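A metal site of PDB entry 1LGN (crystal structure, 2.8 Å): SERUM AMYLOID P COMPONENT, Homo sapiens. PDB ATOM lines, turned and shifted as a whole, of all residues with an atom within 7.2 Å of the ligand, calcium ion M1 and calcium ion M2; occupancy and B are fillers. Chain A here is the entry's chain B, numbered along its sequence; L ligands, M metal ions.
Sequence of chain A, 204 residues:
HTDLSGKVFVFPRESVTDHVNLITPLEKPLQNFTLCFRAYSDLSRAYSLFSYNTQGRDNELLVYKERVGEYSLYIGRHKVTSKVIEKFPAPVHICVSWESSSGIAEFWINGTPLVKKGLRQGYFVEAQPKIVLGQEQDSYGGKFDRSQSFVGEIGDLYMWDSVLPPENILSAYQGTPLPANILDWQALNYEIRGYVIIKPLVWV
Five residues have an atom within 4 Å of calcium ion M2: Asp 58, Asn 59, Glu 136, Gln 137 and Asp 138.
The nearest printed residue that does not touch calcium ion M2 is Asn 53 (4.9 Å).
N of Asn 59 is in hydrogen-bond range of OD1 of Asn 53 (3.1 Å).
OD1 of Asp 58 lies close to ND2 of Asn 53 (3.1 Å).
The side-chain hydroxyl (OH) of Tyr 64 sits at hydrogen-bond distance from the side-chain amide nitrogen (NE2) of Gln 148 (2.8 Å).
N of Asp 138 lies close to O of Lys 143 (3.4 Å).
The side-chain amide oxygen (OE1) of Gln 137 sits close to the backbone carbonyl oxygen (O) of Ser 139.
The side-chain hydroxyl (OG) of Ser 51 lies within hydrogen-bond range of the backbone NH (N) of Gln 137 (3.4 Å).
OH of Tyr 74 lies close to NZ of Lys 79 (3.5 Å).
N of Tyr 74 lies within hydrogen-bond range of O of Leu 62, 2.9 Å away.
Hydrophobic or aromatic side chains within 4 Å of the ligand: Tyr 64.
Nine residues have an atom within 4 Å of the ligand: Asp 58, Asn 59, Tyr 64, Tyr 74, Glu 136, Asp 138, Asp 145, Ser 147 and Gln 148.
OE2 of Glu 136 is bound to calcium ion M2, at 2.3 Å.
The side-chain amide oxygen (OD1) of Asn 59 binds calcium ion M2, at 2.3 Å.
O6 of the ligand is bound to calcium ion M2, at 2.3 Å.
The side-chain carboxylate (OD1) of Asp 58 binds calcium ion M2.
Calcium ion M2 is bound by the side-chain carboxylate (OD1) of Asp 138 (2.4 Å).
Calcium ion M2 is bound by O of Gln 137 (2.5 Å).
OD2 of Asp 58 binds calcium ion M2 (2.8 Å).
Slightly farther from calcium ion M2 lies the side-chain carboxylate (OE1) of Glu 136 (3.0 Å).
N3 of the ligand sits at hydrogen-bond distance from OG of Ser 147 (3.1 Å).
OH of Tyr 64 sits at hydrogen-bond distance from O2 of the ligand.
The side-chain hydroxyl (OH) of Tyr 74 is in hydrogen-bond range of an oxygen (O3) of the ligand, at 3.4 Å.
The side-chain carboxylate (OD2) of Asp 145 binds calcium ion M1 (2.2 Å).
OE1 of Glu 136 binds calcium ion M1, at 2.2 Å.
OE1 of Gln 148 binds calcium ion M1 (2.4 Å).
An oxygen (O5) of the ligand binds calcium ion M1.
Calcium ion M1 is bound by OD2 of Asp 138 (2.5 Å).
The side-chain carboxylate (OD1) of Asp 138 binds calcium ion M1 (2.5 Å).
Within 4 Å of calcium ion M1: Glu 136, Asp 138, Asp 145 and Gln 148.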
ATOM      1  N   ALA A  46      10.040  17.747 -27.465  1.00  0.00           N
ATOM      2  CA  ALA A  46      10.296  17.702 -26.046  1.00  0.00           C
ATOM      3  C   ALA A  46       9.799  19.004 -25.453  1.00  0.00           C
ATOM      4  O   ALA A  46       9.737  20.031 -26.127  1.00  0.00           O
ATOM      5  CB  ALA A  46      11.790  17.574 -25.795  1.00  0.00           C
ATOM      6  N   SER A  51       9.376  23.412 -14.101  1.00  0.00           N
ATOM      7  CA  SER A  51      10.730  23.954 -13.899  1.00  0.00           C
ATOM      8  C   SER A  51      10.873  24.572 -12.524  1.00  0.00           C
ATOM      9  O   SER A  51      10.002  25.310 -12.073  1.00  0.00           O
ATOM     10  CB  SER A  51      11.058  24.987 -14.967  1.00  0.00           C
ATOM     11  OG  SER A  51      12.440  25.267 -14.942  1.00  0.00           O
ATOM     12  N   ASN A  53      14.080  26.404 -10.444  1.00  0.00           N
ATOM     13  CA  ASN A  53      15.455  26.884 -10.359  1.00  0.00           C
ATOM     14  C   ASN A  53      15.674  27.722  -9.116  1.00  0.00           C
ATOM     15  O   ASN A  53      14.752  28.329  -8.600  1.00  0.00           O
ATOM     16  CB  ASN A  53      15.787  27.757 -11.566  1.00  0.00           C
ATOM     17  CG  ASN A  53      16.167  26.954 -12.770  1.00  0.00           C
ATOM     18  OD1 ASN A  53      15.895  25.760 -12.852  1.00  0.00           O
ATOM     19  ND2 ASN A  53      16.845  27.597 -13.711  1.00  0.00           N
ATOM     20  N   ASP A  58      20.897  25.928 -12.184  1.00  0.00           N
ATOM     21  CA  ASP A  58      19.975  25.648 -13.298  1.00  0.00           C
ATOM     22  C   ASP A  58      19.510  24.199 -13.134  1.00  0.00           C
ATOM     23  O   ASP A  58      20.251  23.372 -12.648  1.00  0.00           O
ATOM     24  CB  ASP A  58      20.647  25.835 -14.668  1.00  0.00           C
ATOM     25  CG  ASP A  58      19.689  25.634 -15.867  1.00  0.00           C
ATOM     26  OD1 ASP A  58      18.454  25.785 -15.716  1.00  0.00           O
ATOM     27  OD2 ASP A  58      20.153  25.339 -16.989  1.00  0.00           O
ATOM     28  N   ASN A  59      18.268  23.926 -13.497  1.00  0.00           N
ATOM     29  CA  ASN A  59      17.734  22.583 -13.377  1.00  0.00           C
ATOM     30  C   ASN A  59      17.974  22.032 -11.981  1.00  0.00           C
ATOM     31  O   ASN A  59      18.615  21.008 -11.829  1.00  0.00           O
ATOM     32  CB  ASN A  59      18.358  21.637 -14.407  1.00  0.00           C
ATOM     33  CG  ASN A  59      18.291  22.174 -15.833  1.00  0.00           C
ATOM     34  OD1 ASN A  59      17.416  22.972 -16.183  1.00  0.00           O
ATOM     35  ND2 ASN A  59      19.230  21.751 -16.653  1.00  0.00           N
ATOM     36  N   GLU A  60      17.522  22.745 -10.960  1.00  0.00           N
ATOM     37  CA  GLU A  60      17.693  22.260  -9.598  1.00  0.00           C
ATOM     38  C   GLU A  60      16.708  21.109  -9.415  1.00  0.00           C
ATOM     39  O   GLU A  60      17.017  20.101  -8.811  1.00  0.00           O
ATOM     40  CB  GLU A  60      17.423  23.381  -8.585  1.00  0.00           C
ATOM     41  CG  GLU A  60      17.681  22.998  -7.140  1.00  0.00           C
ATOM     42  CD  GLU A  60      19.111  22.609  -6.872  1.00  0.00           C
ATOM     43  OE1 GLU A  60      19.993  22.833  -7.737  1.00  0.00           O
ATOM     44  OE2 GLU A  60      19.369  22.064  -5.794  1.00  0.00           O
ATOM     45  N   LEU A  62      13.745  19.612 -12.183  1.00  0.00           N
ATOM     46  CA  LEU A  62      13.057  19.711 -13.487  1.00  0.00           C
ATOM     47  C   LEU A  62      12.424  18.398 -13.959  1.00  0.00           C
ATOM     48  O   LEU A  62      13.110  17.381 -14.021  1.00  0.00           O
ATOM     49  CB  LEU A  62      14.071  20.188 -14.540  1.00  0.00           C
ATOM     50  CG  LEU A  62      13.806  20.066 -16.047  1.00  0.00           C
ATOM     51  CD1 LEU A  62      12.638  20.926 -16.465  1.00  0.00           C
ATOM     52  CD2 LEU A  62      15.051  20.466 -16.813  1.00  0.00           C
ATOM     53  N   TYR A  64      11.100  16.913 -17.093  1.00  0.00           N
ATOM     54  CA  TYR A  64      11.160  17.159 -18.534  1.00  0.00           C
ATOM     55  C   TYR A  64      10.713  15.965 -19.355  1.00  0.00           C
ATOM     56  O   TYR A  64      11.058  14.841 -19.026  1.00  0.00           O
ATOM     57  CB  TYR A  64      12.618  17.475 -18.850  1.00  0.00           C
ATOM     58  CG  TYR A  64      12.907  18.075 -20.188  1.00  0.00           C
ATOM     59  CD1 TYR A  64      12.577  19.414 -20.474  1.00  0.00           C
ATOM     60  CD2 TYR A  64      13.572  17.347 -21.165  1.00  0.00           C
ATOM     61  CE1 TYR A  64      12.909  19.998 -21.686  1.00  0.00           C
ATOM     62  CE2 TYR A  64      13.908  17.923 -22.382  1.00  0.00           C
ATOM     63  CZ  TYR A  64      13.587  19.246 -22.632  1.00  0.00           C
ATOM     64  OH  TYR A  64      13.946  19.793 -23.824  1.00  0.00           O
ATOM     65  N   GLU A  66      11.160  13.985 -22.673  1.00  0.00           N
ATOM     66  CA  GLU A  66      12.043  13.742 -23.807  1.00  0.00           C
ATOM     67  C   GLU A  66      11.354  13.476 -25.128  1.00  0.00           C
ATOM     68  O   GLU A  66      11.807  13.937 -26.187  1.00  0.00           O
ATOM     69  CB  GLU A  66      12.916  12.533 -23.476  1.00  0.00           C
ATOM     70  CG  GLU A  66      13.737  12.691 -22.229  1.00  0.00           C
ATOM     71  CD  GLU A  66      14.820  13.756 -22.390  1.00  0.00           C
ATOM     72  OE1 GLU A  66      15.168  14.087 -23.555  1.00  0.00           O
ATOM     73  OE2 GLU A  66      15.315  14.245 -21.349  1.00  0.00           O
ATOM     74  N   TYR A  74      15.373  15.800 -13.228  1.00  0.00           N
ATOM     75  CA  TYR A  74      16.680  16.362 -12.934  1.00  0.00           C
ATOM     76  C   TYR A  74      16.688  16.737 -11.460  1.00  0.00           C
ATOM     77  O   TYR A  74      15.664  17.179 -10.932  1.00  0.00           O
ATOM     78  CB  TYR A  74      16.916  17.632 -13.749  1.00  0.00           C
ATOM     79  CG  TYR A  74      17.256  17.448 -15.206  1.00  0.00           C
ATOM     80  CD1 TYR A  74      16.285  17.066 -16.150  1.00  0.00           C
ATOM     81  CD2 TYR A  74      18.555  17.693 -15.661  1.00  0.00           C
ATOM     82  CE1 TYR A  74      16.604  16.929 -17.508  1.00  0.00           C
ATOM     83  CE2 TYR A  74      18.885  17.566 -17.010  1.00  0.00           C
ATOM     84  CZ  TYR A  74      17.916  17.179 -17.920  1.00  0.00           C
ATOM     85  OH  TYR A  74      18.281  17.049 -19.242  1.00  0.00           O
ATOM     86  N   LYS A  79      20.471  13.808 -13.967  1.00  0.00           N
ATOM     87  CA  LYS A  79      19.282  13.313 -14.638  1.00  0.00           C
ATOM     88  C   LYS A  79      19.016  11.817 -14.696  1.00  0.00           C
ATOM     89  O   LYS A  79      19.939  11.022 -14.777  1.00  0.00           O
ATOM     90  CB  LYS A  79      19.364  13.843 -16.052  1.00  0.00           C
ATOM     91  CG  LYS A  79      18.369  13.335 -17.038  1.00  0.00           C
ATOM     92  CD  LYS A  79      18.823  13.793 -18.408  1.00  0.00           C
ATOM     93  CE  LYS A  79      17.730  13.607 -19.443  1.00  0.00           C
ATOM     94  NZ  LYS A  79      18.216  13.956 -20.810  1.00  0.00           N
ATOM     95  N   GLU A 136      10.851  26.696 -19.778  1.00  0.00           N
ATOM     96  CA  GLU A 136      11.964  26.057 -19.122  1.00  0.00           C
ATOM     97  C   GLU A 136      13.001  27.110 -18.831  1.00  0.00           C
ATOM     98  O   GLU A 136      13.623  27.675 -19.745  1.00  0.00           O
ATOM     99  CB  GLU A 136      12.556  24.947 -19.988  1.00  0.00           C
ATOM    100  CG  GLU A 136      13.401  23.930 -19.230  1.00  0.00           C
ATOM    101  CD  GLU A 136      14.832  24.389 -18.933  1.00  0.00           C
ATOM    102  OE1 GLU A 136      15.493  24.914 -19.858  1.00  0.00           O
ATOM    103  OE2 GLU A 136      15.292  24.205 -17.782  1.00  0.00           O
ATOM    104  N   GLN A 137      13.206  27.356 -17.535  1.00  0.00           N
ATOM    105  CA  GLN A 137      14.171  28.339 -17.061  1.00  0.00           C
ATOM    106  C   GLN A 137      15.597  27.919 -17.279  1.00  0.00           C
ATOM    107  O   GLN A 137      15.947  26.761 -17.108  1.00  0.00           O
ATOM    108  CB  GLN A 137      14.017  28.559 -15.563  1.00  0.00           C
ATOM    109  CG  GLN A 137      12.726  29.131 -15.129  1.00  0.00           C
ATOM    110  CD  GLN A 137      12.583  29.013 -13.646  1.00  0.00           C
ATOM    111  OE1 GLN A 137      13.331  29.624 -12.894  1.00  0.00           O
ATOM    112  NE2 GLN A 137      11.643  28.177 -13.211  1.00  0.00           N
ATOM    113  N   ASP A 138      16.427  28.864 -17.675  1.00  0.00           N
ATOM    114  CA  ASP A 138      17.838  28.596 -17.856  1.00  0.00           C
ATOM    115  C   ASP A 138      18.559  29.614 -16.984  1.00  0.00           C
ATOM    116  O   ASP A 138      19.782  29.742 -16.985  1.00  0.00           O
ATOM    117  CB  ASP A 138      18.231  28.717 -19.333  1.00  0.00           C
ATOM    118  CG  ASP A 138      18.083  27.390 -20.103  1.00  0.00           C
ATOM    119  OD1 ASP A 138      17.740  26.364 -19.466  1.00  0.00           O
ATOM    120  OD2 ASP A 138      18.342  27.384 -21.322  1.00  0.00           O
ATOM    121  N   SER A 139      17.748  30.324 -16.195  1.00  0.00           N
ATOM    122  CA  SER A 139      18.225  31.331 -15.264  1.00  0.00           C
ATOM    123  C   SER A 139      17.214  31.367 -14.119  1.00  0.00           C
ATOM    124  O   SER A 139      16.242  30.610 -14.129  1.00  0.00           O
ATOM    125  CB  SER A 139      18.270  32.700 -15.952  1.00  0.00           C
ATOM    126  OG  SER A 139      16.970  33.178 -16.225  1.00  0.00           O
ATOM    127  N   GLY A 142      14.037  33.045 -15.508  1.00  0.00           N
ATOM    128  CA  GLY A 142      14.046  33.488 -16.888  1.00  0.00           C
ATOM    129  C   GLY A 142      14.824  32.683 -17.919  1.00  0.00           C
ATOM    130  O   GLY A 142      15.049  31.488 -17.750  1.00  0.00           O
ATOM    131  N   LYS A 143      15.274  33.370 -18.968  1.00  0.00           N
ATOM    132  CA  LYS A 143      16.008  32.779 -20.080  1.00  0.00           C
ATOM    133  C   LYS A 143      15.297  31.550 -20.648  1.00  0.00           C
ATOM    134  O   LYS A 143      15.830  30.441 -20.645  1.00  0.00           O
ATOM    135  CB  LYS A 143      17.462  32.509 -19.689  1.00  0.00           C
ATOM    136  N   PHE A 144      14.083  31.766 -21.131  1.00  0.00           N
ATOM    137  CA  PHE A 144      13.233  30.717 -21.703  1.00  0.00           C
ATOM    138  C   PHE A 144      13.623  30.326 -23.116  1.00  0.00           C
ATOM    139  O   PHE A 144      14.049  31.171 -23.896  1.00  0.00           O
ATOM    140  CB  PHE A 144      11.797  31.202 -21.732  1.00  0.00           C
ATOM    141  CG  PHE A 144      11.256  31.559 -20.390  1.00  0.00           C
ATOM    142  CD1 PHE A 144      11.817  31.003 -19.245  1.00  0.00           C
ATOM    143  CD2 PHE A 144      10.171  32.409 -20.261  1.00  0.00           C
ATOM    144  CE1 PHE A 144      11.295  31.297 -17.995  1.00  0.00           C
ATOM    145  CE2 PHE A 144       9.658  32.707 -19.014  1.00  0.00           C
ATOM    146  CZ  PHE A 144      10.217  32.145 -17.882  1.00  0.00           C
ATOM    147  N   ASP A 145      13.520  29.021 -23.425  1.00  0.00           N
ATOM    148  CA  ASP A 145      13.825  28.483 -24.759  1.00  0.00           C
ATOM    149  C   ASP A 145      12.473  28.136 -25.384  1.00  0.00           C
ATOM    150  O   ASP A 145      11.680  27.403 -24.768  1.00  0.00           O
ATOM    151  CB  ASP A 145      14.705  27.225 -24.689  1.00  0.00           C
ATOM    152  CG  ASP A 145      16.196  27.523 -24.385  1.00  0.00           C
ATOM    153  OD1 ASP A 145      16.877  28.141 -25.229  1.00  0.00           O
ATOM    154  OD2 ASP A 145      16.701  27.099 -23.306  1.00  0.00           O
ATOM    155  N   ARG A 146      12.199  28.675 -26.574  1.00  0.00           N
ATOM    156  CA  ARG A 146      10.910  28.434 -27.233  1.00  0.00           C
ATOM    157  C   ARG A 146      10.667  26.986 -27.574  1.00  0.00           C
ATOM    158  O   ARG A 146       9.537  26.514 -27.530  1.00  0.00           O
ATOM    159  CB  ARG A 146      10.800  29.266 -28.509  1.00  0.00           C
ATOM    160  CG  ARG A 146       9.652  28.836 -29.419  1.00  0.00           C
ATOM    161  CD  ARG A 146       9.759  29.437 -30.799  1.00  0.00           C
ATOM    162  NE  ARG A 146       8.988  30.680 -30.911  1.00  0.00           N
ATOM    163  CZ  ARG A 146       7.692  30.737 -31.200  1.00  0.00           C
ATOM    164  NH1 ARG A 146       6.992  29.624 -31.400  1.00  0.00           N
ATOM    165  NH2 ARG A 146       7.091  31.909 -31.299  1.00  0.00           N
ATOM    166  N   SER A 147      11.730  26.275 -27.918  1.00  0.00           N
ATOM    167  CA  SER A 147      11.654  24.870 -28.289  1.00  0.00           C
ATOM    168  C   SER A 147      11.413  23.928 -27.120  1.00  0.00           C
ATOM    169  O   SER A 147      11.289  22.715 -27.303  1.00  0.00           O
ATOM    170  CB  SER A 147      12.910  24.453 -29.045  1.00  0.00           C
ATOM    171  OG  SER A 147      14.075  24.937 -28.388  1.00  0.00           O
ATOM    172  N   GLN A 148      11.354  24.491 -25.914  1.00  0.00           N
ATOM    173  CA  GLN A 148      11.094  23.704 -24.717  1.00  0.00           C
ATOM    174  C   GLN A 148       9.768  24.094 -24.087  1.00  0.00           C
ATOM    175  O   GLN A 148       9.316  23.472 -23.144  1.00  0.00           O
ATOM    176  CB  GLN A 148      12.239  23.846 -23.725  1.00  0.00           C
ATOM    177  CG  GLN A 148      13.518  23.296 -24.253  1.00  0.00           C
ATOM    178  CD  GLN A 148      14.615  23.335 -23.247  1.00  0.00           C
ATOM    179  OE1 GLN A 148      14.906  24.373 -22.668  1.00  0.00           O
ATOM    180  NE2 GLN A 148      15.254  22.189 -23.041  1.00  0.00           N
HETATM  181  O1  LIG L   1      18.627  21.462 -20.848  1.00  0.00           O
HETATM  182  C1  LIG L   1      17.554  20.576 -20.643  1.00  0.00           C
HETATM  183  C2  LIG L   1      17.625  19.513 -21.730  1.00  0.00           C
HETATM  184  O2  LIG L   1      17.055  20.017 -22.936  1.00  0.00           O
HETATM  185  C3  LIG L   1      19.061  19.170 -22.070  1.00  0.00           C
HETATM  186  O3  LIG L   1      19.112  17.807 -22.425  1.00  0.00           O
HETATM  187  C4  LIG L   1      19.381  19.973 -23.307  1.00  0.00           C
HETATM  188  C5  LIG L   1      18.051  20.126 -23.963  1.00  0.00           C
HETATM  189  N1  LIG L   1      17.934  21.438 -24.592  1.00  0.00           N
HETATM  190  C6  LIG L   1      18.229  22.669 -24.092  1.00  0.00           C
HETATM  191  N2  LIG L   1      18.001  23.666 -24.899  1.00  0.00           N
HETATM  192  C7  LIG L   1      17.514  23.033 -26.018  1.00  0.00           C
HETATM  193  C8  LIG L   1      17.081  23.510 -27.273  1.00  0.00           C
HETATM  194  N3  LIG L   1      17.080  24.813 -27.611  1.00  0.00           N
HETATM  195  N4  LIG L   1      16.664  22.607 -28.189  1.00  0.00           N
HETATM  196  C9  LIG L   1      16.673  21.308 -27.854  1.00  0.00           C
HETATM  197  N5  LIG L   1      17.054  20.747 -26.695  1.00  0.00           N
HETATM  198  C10 LIG L   1      17.467  21.664 -25.831  1.00  0.00           C
HETATM  199  P1  LIG L   1      18.649  23.015 -20.456  1.00  0.00           P
HETATM  200  O4  LIG L   1      20.056  23.429 -20.746  1.00  0.00           O
HETATM  201  O5  LIG L   1      17.640  23.744 -21.341  1.00  0.00           O
HETATM  202  O6  LIG L   1      18.343  23.096 -18.982  1.00  0.00           O
HETATM  203 CA    CA M   1      16.453  25.813 -21.583  1.00  0.00          CA
HETATM  204 CA    CA M   2      17.472  24.796 -17.638  1.00  0.00          CA
